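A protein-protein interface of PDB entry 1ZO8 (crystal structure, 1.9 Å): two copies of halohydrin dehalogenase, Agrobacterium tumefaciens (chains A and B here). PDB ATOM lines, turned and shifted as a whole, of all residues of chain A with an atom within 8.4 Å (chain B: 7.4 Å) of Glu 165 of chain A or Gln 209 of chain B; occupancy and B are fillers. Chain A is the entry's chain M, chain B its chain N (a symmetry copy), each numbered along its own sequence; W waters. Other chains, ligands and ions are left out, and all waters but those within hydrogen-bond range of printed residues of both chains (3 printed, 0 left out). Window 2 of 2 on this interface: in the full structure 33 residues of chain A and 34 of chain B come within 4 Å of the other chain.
Water W2 lies within hydrogen-bond range of O of Lys 161 of chain A, O of Ala 207 of chain B and N of Glu 165 of chain A.
Water W1 lies within hydrogen-bond range of the side-chain amide oxygen of Asn 167 of chain A (2.7 Å) and the guanidinium group of Arg 210 of chain B (2.9 Å).
Water W3 lies within hydrogen-bond range of OD1 of Asn 167 of chain A (2.7 Å) and NE of Arg 210 of chain B (2.9 Å).
No position is printed for both chains.
Of the 14 pairs that touch across the chains among the printed residues, none has its exchanged pair printed and touching as well.
The side-chain amide nitrogen (NE2) of Gln 209 of chain B lies close to the backbone carbonyl oxygen (O) of Lys 203 of chain B (3.3 Å).
The backbone NH of Leu 208 of chain B is in hydrogen-bond range of the backbone carbonyl oxygen of Gly 241 of chain B, at 3.0 Å.
The backbone carbonyl oxygen (O) of Val 202 of chain B lies within hydrogen-bond range of the side-chain hydroxyl (OG1) of Thr 206 of chain B, at 2.8 Å.
The backbone carbonyl oxygen (O) of Val 205 of chain B is in hydrogen-bond range of the backbone NH (N) of Met 245 of chain B (3.1 Å).
The side-chain hydroxyl (OG1) of Thr 206 of chain B sits at hydrogen-bond distance from the backbone NH (N) of Arg 210 of chain B.
The backbone carbonyl oxygen (O) of Gly 241 of chain B lies within hydrogen-bond range of the backbone NH (N) of Ala 207 of chain B (2.9 Å).
Glu 162 of chain A touches none of the printed residues of chain B.
Glu 165 of chain A touches just these residues of chain B: Ala 207 and Gln 209.
Gln 209 of chain B touches one residue of chain A.
Printed residues of chain A within 4 Å of Arg 210 of chain B: Tyr 231.
Of the printed residues of chain A, Leu 211 of chain B touches Tyr 231 (3.6 Å).
The nearest residue of chain B that does not touch Glu 165 of chain A is Leu 208 of chain B (4.9 Å).
The nearest residue of chain A that does not touch Gln 209 of chain B is Gly 164 of chain A (5.1 Å).
Ser 160 of chain A touches Ala 207 of chain B (O to CB, 3.6 Å).
Lys 161 of chain A touches Met 245 of chain B.
Gly 164 of chain A touches Leu 208 of chain B.
OE1 of Gln 209 of chain B touches CG of Glu 165 of chain A, at 3.6 Å.
OH of Tyr 231 of chain A touches CG2 of Thr 206 of chain B (3.7 Å).
Leu 208 of chain B touches Tyr 231 of chain A (CD1 to CD2, 3.8 Å).
Tyr 231 of chain A touches Leu 211 of chain B (OH to C, 3.6 Å).
Thr 233 of chain A touches Gly 241 of chain B (CG2 to C, 3.6 Å).
Gly 242 of chain B touches Thr 233 of chain A.
Hydrophobic or aromatic side chains of chain A that line the printed part of chain B: Tyr 231.
Hydrophobic or aromatic side chains of chain B that line the printed part of chain A: Ala 207, Leu 208 and Met 245.
Among the printed residues, 14 pairs touch across the chains.
Among the printed residues, no Asp or Glu carboxylate lies within 4 Å of a Lys or Arg side-chain nitrogen of the other chain.
The side-chain amino group of Lys 161 of chain A lies within hydrogen-bond range of the backbone carbonyl oxygen of Gly 242 of chain B, at 2.7 Å.
O of Tyr 231 of chain A sits at hydrogen-bond distance from N of Gly 241 of chain B (2.8 Å).
The backbone carbonyl oxygen (O) of Arg 210 of chain B sits at hydrogen-bond distance from the side-chain hydroxyl (OH) of Tyr 231 of chain A (2.7 Å).
O of Ala 207 of chain B lies close to O of Gly 164 of chain A, 3.4 Å away.
The backbone NH of Glu 165 of chain A sits at hydrogen-bond distance from the backbone carbonyl oxygen of Ala 207 of chain B, 3.2 Å away.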
ATOM      1  N   LYS A 120       5.577  11.417  -1.452  1.00  0.00           N
ATOM      2  CA  LYS A 120       4.887  10.660  -2.493  1.00  0.00           C
ATOM      3  C   LYS A 120       4.032   9.516  -1.967  1.00  0.00           C
ATOM      4  O   LYS A 120       3.000   9.181  -2.557  1.00  0.00           O
ATOM      5  CB  LYS A 120       5.888  10.120  -3.515  1.00  0.00           C
ATOM      6  CG  LYS A 120       6.433  11.195  -4.451  1.00  0.00           C
ATOM      7  CD  LYS A 120       7.621  10.705  -5.266  1.00  0.00           C
ATOM      8  CE  LYS A 120       7.240   9.558  -6.183  1.00  0.00           C
ATOM      9  NZ  LYS A 120       8.385   9.162  -7.052  1.00  0.00           N
ATOM     10  N   LYS A 123       1.108  11.153  -0.590  1.00  0.00           N
ATOM     11  CA  LYS A 123       0.484  11.943  -1.649  1.00  0.00           C
ATOM     12  C   LYS A 123       0.116  13.330  -1.125  1.00  0.00           C
ATOM     13  O   LYS A 123      -0.985  13.828  -1.374  1.00  0.00           O
ATOM     14  CB  LYS A 123      -0.762  11.250  -2.206  1.00  0.00           C
ATOM     15  CG  LYS A 123      -0.454  10.048  -3.084  1.00  0.00           C
ATOM     16  CD  LYS A 123      -1.695   9.541  -3.808  1.00  0.00           C
ATOM     17  CE  LYS A 123      -1.367   8.324  -4.667  1.00  0.00           C
ATOM     18  NZ  LYS A 123      -2.549   7.834  -5.441  1.00  0.00           N
ATOM     19  N   SER A 124       1.038  13.939  -0.385  1.00  0.00           N
ATOM     20  CA  SER A 124       0.832  15.283   0.149  1.00  0.00           C
ATOM     21  C   SER A 124       2.166  15.917   0.528  1.00  0.00           C
ATOM     22  O   SER A 124       3.041  15.267   1.113  1.00  0.00           O
ATOM     23  CB  SER A 124      -0.082  15.261   1.376  1.00  0.00           C
ATOM     24  OG  SER A 124       0.647  14.930   2.545  1.00  0.00           O
ATOM     25  N   LEU A 159      10.477  19.298 -11.678  1.00  0.00           N
ATOM     26  CA  LEU A 159       9.968  18.482 -10.576  1.00  0.00           C
ATOM     27  C   LEU A 159       8.443  18.533 -10.472  1.00  0.00           C
ATOM     28  O   LEU A 159       7.797  17.522 -10.161  1.00  0.00           O
ATOM     29  CB  LEU A 159      10.598  18.935  -9.253  1.00  0.00           C
ATOM     30  CG  LEU A 159      12.079  18.561  -9.111  1.00  0.00           C
ATOM     31  CD1 LEU A 159      12.637  19.110  -7.809  1.00  0.00           C
ATOM     32  CD2 LEU A 159      12.228  17.046  -9.162  1.00  0.00           C
ATOM     33  N   SER A 160       7.866  19.703 -10.735  1.00  0.00           N
ATOM     34  CA  SER A 160       6.417  19.853 -10.663  1.00  0.00           C
ATOM     35  C   SER A 160       5.732  18.862 -11.599  1.00  0.00           C
ATOM     36  O   SER A 160       4.659  18.334 -11.284  1.00  0.00           O
ATOM     37  CB  SER A 160       6.002  21.286 -11.033  1.00  0.00           C
ATOM     38  OG  SER A 160       6.107  21.507 -12.428  1.00  0.00           O
ATOM     39  N   LYS A 161       6.354  18.597 -12.744  1.00  0.00           N
ATOM     40  CA  LYS A 161       5.786  17.679 -13.725  1.00  0.00           C
ATOM     41  C   LYS A 161       5.582  16.262 -13.189  1.00  0.00           C
ATOM     42  O   LYS A 161       4.578  15.619 -13.493  1.00  0.00           O
ATOM     43  CB  LYS A 161       6.667  17.609 -14.975  1.00  0.00           C
ATOM     44  CG  LYS A 161       6.925  18.950 -15.659  1.00  0.00           C
ATOM     45  CD  LYS A 161       5.641  19.629 -16.099  1.00  0.00           C
ATOM     46  CE  LYS A 161       5.954  20.912 -16.864  1.00  0.00           C
ATOM     47  NZ  LYS A 161       4.737  21.634 -17.335  1.00  0.00           N
ATOM     48  N   GLU A 162       6.528  15.771 -12.400  1.00  0.00           N
ATOM     49  CA  GLU A 162       6.409  14.418 -11.870  1.00  0.00           C
ATOM     50  C   GLU A 162       5.748  14.318 -10.505  1.00  0.00           C
ATOM     51  O   GLU A 162       5.095  13.321 -10.211  1.00  0.00           O
ATOM     52  CB  GLU A 162       7.788  13.746 -11.814  1.00  0.00           C
ATOM     53  CG  GLU A 162       8.776  14.394 -10.857  1.00  0.00           C
ATOM     54  CD  GLU A 162      10.111  13.670 -10.836  1.00  0.00           C
ATOM     55  OE1 GLU A 162      10.242  12.642 -10.136  1.00  0.00           O
ATOM     56  OE2 GLU A 162      11.030  14.133 -11.539  1.00  0.00           O
ATOM     57  N   LEU A 163       5.912  15.335  -9.665  1.00  0.00           N
ATOM     58  CA  LEU A 163       5.324  15.286  -8.336  1.00  0.00           C
ATOM     59  C   LEU A 163       3.833  15.633  -8.309  1.00  0.00           C
ATOM     60  O   LEU A 163       3.139  15.322  -7.344  1.00  0.00           O
ATOM     61  CB  LEU A 163       6.114  16.190  -7.377  1.00  0.00           C
ATOM     62  CG  LEU A 163       7.590  15.789  -7.197  1.00  0.00           C
ATOM     63  CD1 LEU A 163       8.271  16.713  -6.204  1.00  0.00           C
ATOM     64  CD2 LEU A 163       7.664  14.347  -6.711  1.00  0.00           C
ATOM     65  N   GLY A 164       3.343  16.262  -9.375  1.00  0.00           N
ATOM     66  CA  GLY A 164       1.934  16.620  -9.433  1.00  0.00           C
ATOM     67  C   GLY A 164       1.031  15.395  -9.382  1.00  0.00           C
ATOM     68  O   GLY A 164      -0.083  15.456  -8.860  1.00  0.00           O
ATOM     69  N   GLU A 165       1.522  14.285  -9.926  1.00  0.00           N
ATOM     70  CA  GLU A 165       0.774  13.030  -9.956  1.00  0.00           C
ATOM     71  C   GLU A 165       0.562  12.509  -8.540  1.00  0.00           C
ATOM     72  O   GLU A 165      -0.316  11.681  -8.293  1.00  0.00           O
ATOM     73  CB  GLU A 165       1.540  11.991 -10.773  1.00  0.00           C
ATOM     74  CG  GLU A 165       0.752  10.735 -11.083  1.00  0.00           C
ATOM     75  CD  GLU A 165       1.607   9.653 -11.712  1.00  0.00           C
ATOM     76  OE1 GLU A 165       1.029   8.665 -12.209  1.00  0.00           O
ATOM     77  OE2 GLU A 165       2.848   9.782 -11.702  1.00  0.00           O
ATOM     78  N   TYR A 166       1.377  13.009  -7.616  1.00  0.00           N
ATOM     79  CA  TYR A 166       1.318  12.623  -6.215  1.00  0.00           C
ATOM     80  C   TYR A 166       0.782  13.774  -5.383  1.00  0.00           C
ATOM     81  O   TYR A 166       0.955  13.808  -4.166  1.00  0.00           O
ATOM     82  CB  TYR A 166       2.711  12.229  -5.732  1.00  0.00           C
ATOM     83  CG  TYR A 166       3.237  10.990  -6.423  1.00  0.00           C
ATOM     84  CD1 TYR A 166       3.010   9.722  -5.888  1.00  0.00           C
ATOM     85  CD2 TYR A 166       3.910  11.082  -7.640  1.00  0.00           C
ATOM     86  CE1 TYR A 166       3.439   8.574  -6.548  1.00  0.00           C
ATOM     87  CE2 TYR A 166       4.343   9.938  -8.312  1.00  0.00           C
ATOM     88  CZ  TYR A 166       4.102   8.689  -7.759  1.00  0.00           C
ATOM     89  OH  TYR A 166       4.507   7.553  -8.422  1.00  0.00           O
ATOM     90  N   ASN A 167       0.141  14.725  -6.058  1.00  0.00           N
ATOM     91  CA  ASN A 167      -0.445  15.885  -5.401  1.00  0.00           C
ATOM     92  C   ASN A 167       0.589  16.703  -4.638  1.00  0.00           C
ATOM     93  O   ASN A 167       0.320  17.196  -3.544  1.00  0.00           O
ATOM     94  CB  ASN A 167      -1.573  15.442  -4.455  1.00  0.00           C
ATOM     95  CG  ASN A 167      -2.450  16.602  -4.007  1.00  0.00           C
ATOM     96  OD1 ASN A 167      -2.969  17.352  -4.831  1.00  0.00           O
ATOM     97  ND2 ASN A 167      -2.624  16.747  -2.699  1.00  0.00           N
ATOM     98  N   ILE A 168       1.772  16.855  -5.226  1.00  0.00           N
ATOM     99  CA  ILE A 168       2.835  17.620  -4.593  1.00  0.00           C
ATOM    100  C   ILE A 168       3.214  18.813  -5.456  1.00  0.00           C
ATOM    101  O   ILE A 168       3.862  18.648  -6.485  1.00  0.00           O
ATOM    102  CB  ILE A 168       4.110  16.776  -4.398  1.00  0.00           C
ATOM    103  CG1 ILE A 168       3.770  15.478  -3.664  1.00  0.00           C
ATOM    104  CG2 ILE A 168       5.148  17.583  -3.626  1.00  0.00           C
ATOM    105  CD1 ILE A 168       3.042  15.681  -2.380  1.00  0.00           C
ATOM    106  N   PRO A 169       2.793  20.022  -5.061  1.00  0.00           N
ATOM    107  CA  PRO A 169       3.121  21.228  -5.830  1.00  0.00           C
ATOM    108  C   PRO A 169       4.588  21.595  -5.583  1.00  0.00           C
ATOM    109  O   PRO A 169       5.108  21.399  -4.480  1.00  0.00           O
ATOM    110  CB  PRO A 169       2.181  22.282  -5.244  1.00  0.00           C
ATOM    111  CG  PRO A 169       1.035  21.467  -4.662  1.00  0.00           C
ATOM    112  CD  PRO A 169       1.784  20.326  -4.030  1.00  0.00           C
ATOM    113  N   TYR A 231      -2.721  24.737  -7.782  1.00  0.00           N
ATOM    114  CA  TYR A 231      -2.784  24.729  -9.239  1.00  0.00           C
ATOM    115  C   TYR A 231      -1.702  25.582  -9.898  1.00  0.00           C
ATOM    116  O   TYR A 231      -1.565  25.578 -11.122  1.00  0.00           O
ATOM    117  CB  TYR A 231      -4.170  25.167  -9.720  1.00  0.00           C
ATOM    118  CG  TYR A 231      -4.657  24.358 -10.901  1.00  0.00           C
ATOM    119  CD1 TYR A 231      -4.929  24.964 -12.123  1.00  0.00           C
ATOM    120  CD2 TYR A 231      -4.815  22.971 -10.800  1.00  0.00           C
ATOM    121  CE1 TYR A 231      -5.345  24.214 -13.220  1.00  0.00           C
ATOM    122  CE2 TYR A 231      -5.228  22.213 -11.889  1.00  0.00           C
ATOM    123  CZ  TYR A 231      -5.492  22.838 -13.095  1.00  0.00           C
ATOM    124  OH  TYR A 231      -5.903  22.092 -14.177  1.00  0.00           O
ATOM    125  N   THR A 233       1.343  25.020  -9.428  1.00  0.00           N
ATOM    126  CA  THR A 233       2.536  24.178  -9.459  1.00  0.00           C
ATOM    127  C   THR A 233       3.393  24.346 -10.715  1.00  0.00           C
ATOM    128  O   THR A 233       2.873  24.425 -11.831  1.00  0.00           O
ATOM    129  CB  THR A 233       2.189  22.682  -9.291  1.00  0.00           C
ATOM    130  OG1 THR A 233       3.405  21.949  -9.102  1.00  0.00           O
ATOM    131  CG2 THR A 233       1.475  22.137 -10.533  1.00  0.00           C
ATOM    132  N   VAL B 199     -12.524  13.790 -19.294  1.00  0.00           N
ATOM    133  CA  VAL B 199     -11.953  13.540 -17.975  1.00  0.00           C
ATOM    134  C   VAL B 199     -10.557  12.935 -18.099  1.00  0.00           C
ATOM    135  O   VAL B 199      -9.641  13.293 -17.355  1.00  0.00           O
ATOM    136  CB  VAL B 199     -12.842  12.574 -17.169  1.00  0.00           C
ATOM    137  CG1 VAL B 199     -12.239  12.334 -15.792  1.00  0.00           C
ATOM    138  CG2 VAL B 199     -14.250  13.141 -17.052  1.00  0.00           C
ATOM    139  N   HIS B 201      -8.595  13.217 -20.715  1.00  0.00           N
ATOM    140  CA  HIS B 201      -7.752  14.233 -21.328  1.00  0.00           C
ATOM    141  C   HIS B 201      -7.106  15.107 -20.258  1.00  0.00           C
ATOM    142  O   HIS B 201      -5.912  15.387 -20.312  1.00  0.00           O
ATOM    143  CB  HIS B 201      -8.587  15.104 -22.260  1.00  0.00           C
ATOM    144  CG  HIS B 201      -7.848  16.279 -22.819  1.00  0.00           C
ATOM    145  ND1 HIS B 201      -6.864  16.155 -23.776  1.00  0.00           N
ATOM    146  CD2 HIS B 201      -7.951  17.603 -22.555  1.00  0.00           C
ATOM    147  CE1 HIS B 201      -6.394  17.352 -24.078  1.00  0.00           C
ATOM    148  NE2 HIS B 201      -7.036  18.248 -23.351  1.00  0.00           N
ATOM    149  N   VAL B 202      -7.905  15.530 -19.282  1.00  0.00           N
ATOM    150  CA  VAL B 202      -7.419  16.387 -18.207  1.00  0.00           C
ATOM    151  C   VAL B 202      -6.377  15.695 -17.334  1.00  0.00           C
ATOM    152  O   VAL B 202      -5.406  16.318 -16.901  1.00  0.00           O
ATOM    153  CB  VAL B 202      -8.590  16.873 -17.322  1.00  0.00           C
ATOM    154  CG1 VAL B 202      -8.071  17.773 -16.217  1.00  0.00           C
ATOM    155  CG2 VAL B 202      -9.605  17.619 -18.176  1.00  0.00           C
ATOM    156  N   LYS B 203      -6.582  14.408 -17.069  1.00  0.00           N
ATOM    157  CA  LYS B 203      -5.643  13.654 -16.249  1.00  0.00           C
ATOM    158  C   LYS B 203      -4.327  13.489 -17.003  1.00  0.00           C
ATOM    159  O   LYS B 203      -3.270  13.318 -16.400  1.00  0.00           O
ATOM    160  CB  LYS B 203      -6.230  12.281 -15.899  1.00  0.00           C
ATOM    161  N   LYS B 204      -4.403  13.557 -18.326  1.00  0.00           N
ATOM    162  CA  LYS B 204      -3.228  13.402 -19.173  1.00  0.00           C
ATOM    163  C   LYS B 204      -2.405  14.682 -19.368  1.00  0.00           C
ATOM    164  O   LYS B 204      -1.181  14.671 -19.224  1.00  0.00           O
ATOM    165  CB  LYS B 204      -3.653  12.869 -20.544  1.00  0.00           C
ATOM    166  CG  LYS B 204      -2.507  12.605 -21.522  1.00  0.00           C
ATOM    167  CD  LYS B 204      -3.027  11.972 -22.810  1.00  0.00           C
ATOM    168  CE  LYS B 204      -1.905  11.476 -23.720  1.00  0.00           C
ATOM    169  NZ  LYS B 204      -1.100  12.572 -24.319  1.00  0.00           N
ATOM    170  N   VAL B 205      -3.083  15.784 -19.677  1.00  0.00           N
ATOM    171  CA  VAL B 205      -2.399  17.043 -19.956  1.00  0.00           C
ATOM    172  C   VAL B 205      -1.964  17.944 -18.802  1.00  0.00           C
ATOM    173  O   VAL B 205      -1.190  18.876 -19.020  1.00  0.00           O
ATOM    174  CB  VAL B 205      -3.222  17.891 -20.946  1.00  0.00           C
ATOM    175  CG1 VAL B 205      -3.434  17.112 -22.237  1.00  0.00           C
ATOM    176  CG2 VAL B 205      -4.548  18.269 -20.324  1.00  0.00           C
ATOM    177  N   THR B 206      -2.453  17.690 -17.592  1.00  0.00           N
ATOM    178  CA  THR B 206      -2.062  18.504 -16.441  1.00  0.00           C
ATOM    179  C   THR B 206      -1.244  17.652 -15.472  1.00  0.00           C
ATOM    180  O   THR B 206      -1.464  16.447 -15.369  1.00  0.00           O
ATOM    181  CB  THR B 206      -3.296  19.076 -15.694  1.00  0.00           C
ATOM    182  OG1 THR B 206      -4.089  18.002 -15.171  1.00  0.00           O
ATOM    183  CG2 THR B 206      -4.154  19.916 -16.640  1.00  0.00           C
ATOM    184  N   ALA B 207      -0.295  18.270 -14.775  1.00  0.00           N
ATOM    185  CA  ALA B 207       0.537  17.536 -13.829  1.00  0.00           C
ATOM    186  C   ALA B 207      -0.276  17.039 -12.643  1.00  0.00           C
ATOM    187  O   ALA B 207      -0.097  15.912 -12.180  1.00  0.00           O
ATOM    188  CB  ALA B 207       1.681  18.418 -13.340  1.00  0.00           C
ATOM    189  N   LEU B 208      -1.169  17.887 -12.146  1.00  0.00           N
ATOM    190  CA  LEU B 208      -1.999  17.528 -11.007  1.00  0.00           C
ATOM    191  C   LEU B 208      -3.141  16.589 -11.393  1.00  0.00           C
ATOM    192  O   LEU B 208      -3.864  16.092 -10.527  1.00  0.00           O
ATOM    193  CB  LEU B 208      -2.549  18.790 -10.347  1.00  0.00           C
ATOM    194  CG  LEU B 208      -1.513  19.619  -9.585  1.00  0.00           C
ATOM    195  CD1 LEU B 208      -2.139  20.935  -9.109  1.00  0.00           C
ATOM    196  CD2 LEU B 208      -1.005  18.810  -8.394  1.00  0.00           C
ATOM    197  N   GLN B 209      -3.297  16.368 -12.695  1.00  0.00           N
ATOM    198  CA  GLN B 209      -4.314  15.470 -13.237  1.00  0.00           C
ATOM    199  C   GLN B 209      -5.733  15.786 -12.782  1.00  0.00           C
ATOM    200  O   GLN B 209      -6.476  14.900 -12.351  1.00  0.00           O
ATOM    201  CB  GLN B 209      -3.968  14.023 -12.876  1.00  0.00           C
ATOM    202  CG  GLN B 209      -2.569  13.616 -13.305  1.00  0.00           C
ATOM    203  CD  GLN B 209      -2.300  12.139 -13.104  1.00  0.00           C
ATOM    204  OE1 GLN B 209      -2.591  11.580 -12.045  1.00  0.00           O
ATOM    205  NE2 GLN B 209      -1.731  11.500 -14.117  1.00  0.00           N
ATOM    206  N   ARG B 210      -6.108  17.053 -12.899  1.00  0.00           N
ATOM    207  CA  ARG B 210      -7.437  17.497 -12.511  1.00  0.00           C
ATOM    208  C   ARG B 210      -7.648  18.914 -13.020  1.00  0.00           C
ATOM    209  O   ARG B 210      -6.710  19.555 -13.490  1.00  0.00           O
ATOM    210  CB  ARG B 210      -7.587  17.483 -10.988  1.00  0.00           C
ATOM    211  CG  ARG B 210      -6.719  18.506 -10.246  1.00  0.00           C
ATOM    212  CD  ARG B 210      -7.075  18.555  -8.769  1.00  0.00           C
ATOM    213  NE  ARG B 210      -6.206  19.424  -7.976  1.00  0.00           N
ATOM    214  CZ  ARG B 210      -6.249  20.755  -7.975  1.00  0.00           C
ATOM    215  NH1 ARG B 210      -7.122  21.407  -8.738  1.00  0.00           N
ATOM    216  NH2 ARG B 210      -5.433  21.438  -7.180  1.00  0.00           N
ATOM    217  N   LEU B 211      -8.885  19.395 -12.938  1.00  0.00           N
ATOM    218  CA  LEU B 211      -9.202  20.752 -13.361  1.00  0.00           C
ATOM    219  C   LEU B 211      -8.886  21.691 -12.211  1.00  0.00           C
ATOM    220  O   LEU B 211      -8.894  21.285 -11.047  1.00  0.00           O
ATOM    221  CB  LEU B 211     -10.691  20.890 -13.690  1.00  0.00           C
ATOM    222  CG  LEU B 211     -11.273  20.201 -14.923  1.00  0.00           C
ATOM    223  CD1 LEU B 211     -12.786  20.392 -14.922  1.00  0.00           C
ATOM    224  CD2 LEU B 211     -10.665  20.779 -16.184  1.00  0.00           C
ATOM    225  N   GLY B 241      -2.201  23.984 -13.391  1.00  0.00           N
ATOM    226  CA  GLY B 241      -1.904  22.696 -12.783  1.00  0.00           C
ATOM    227  C   GLY B 241      -0.758  21.877 -13.340  1.00  0.00           C
ATOM    228  O   GLY B 241      -0.784  20.648 -13.275  1.00  0.00           O
ATOM    229  N   GLY B 242       0.256  22.536 -13.883  1.00  0.00           N
ATOM    230  CA  GLY B 242       1.378  21.786 -14.415  1.00  0.00           C
ATOM    231  C   GLY B 242       1.322  21.617 -15.914  1.00  0.00           C
ATOM    232  O   GLY B 242       2.250  21.078 -16.517  1.00  0.00           O
ATOM    233  N   MET B 245       1.715  18.924 -20.076  1.00  0.00           N
ATOM    234  CA  MET B 245       2.473  17.703 -19.826  1.00  0.00           C
ATOM    235  C   MET B 245       2.888  17.258 -21.216  1.00  0.00           C
ATOM    236  O   MET B 245       2.065  17.198 -22.127  1.00  0.00           O
ATOM    237  CB  MET B 245       1.600  16.639 -19.152  1.00  0.00           C
ATOM    238  CG  MET B 245       1.289  16.928 -17.693  1.00  0.00           C
ATOM    239  SD  MET B 245       2.780  16.989 -16.670  1.00  0.00           S
ATOM    240  CE  MET B 245       3.239  15.276 -16.698  1.00  0.00           C
ATOM    241  N   ARG B 248       5.912  11.635 -23.613  1.00  0.00           N
ATOM    242  CA  ARG B 248       7.208  10.994 -23.433  1.00  0.00           C
ATOM    243  C   ARG B 248       7.442   9.891 -24.457  1.00  0.00           C
ATOM    244  O   ARG B 248       6.535   9.509 -25.199  1.00  0.00           O
ATOM    245  CB  ARG B 248       7.336  10.417 -22.022  1.00  0.00           C
ATOM    246  CG  ARG B 248       7.215  11.457 -20.917  1.00  0.00           C
ATOM    247  CD  ARG B 248       7.866  10.983 -19.624  1.00  0.00           C
ATOM    248  NE  ARG B 248       7.206   9.808 -19.064  1.00  0.00           N
ATOM    249  CZ  ARG B 248       7.657   9.130 -18.013  1.00  0.00           C
ATOM    250  NH1 ARG B 248       8.777   9.507 -17.409  1.00  0.00           N
ATOM    251  NH2 ARG B 248       6.979   8.081 -17.558  1.00  0.00           N
ATOM    252  N   PRO B 253       5.500   4.546 -19.032  1.00  0.00           N
ATOM    253  CA  PRO B 253       4.151   4.598 -18.462  1.00  0.00           C
ATOM    254  C   PRO B 253       3.642   6.024 -18.259  1.00  0.00           C
ATOM    255  O   PRO B 253       4.404   6.965 -18.560  1.00  0.00           O
ATOM    256  CB  PRO B 253       4.312   3.847 -17.148  1.00  0.00           C
ATOM    257  CG  PRO B 253       5.700   4.203 -16.741  1.00  0.00           C
ATOM    258  CD  PRO B 253       6.461   4.031 -18.042  1.00  0.00           C
HETATM  259  O   HOH W   1      -4.094  19.785  -5.147  1.00  0.00           O
HETATM  260  O   HOH W   2       2.316  14.529 -12.694  1.00  0.00           O
HETATM  261  O   HOH W   3      -4.282  17.427  -7.237  1.00  0.00           O
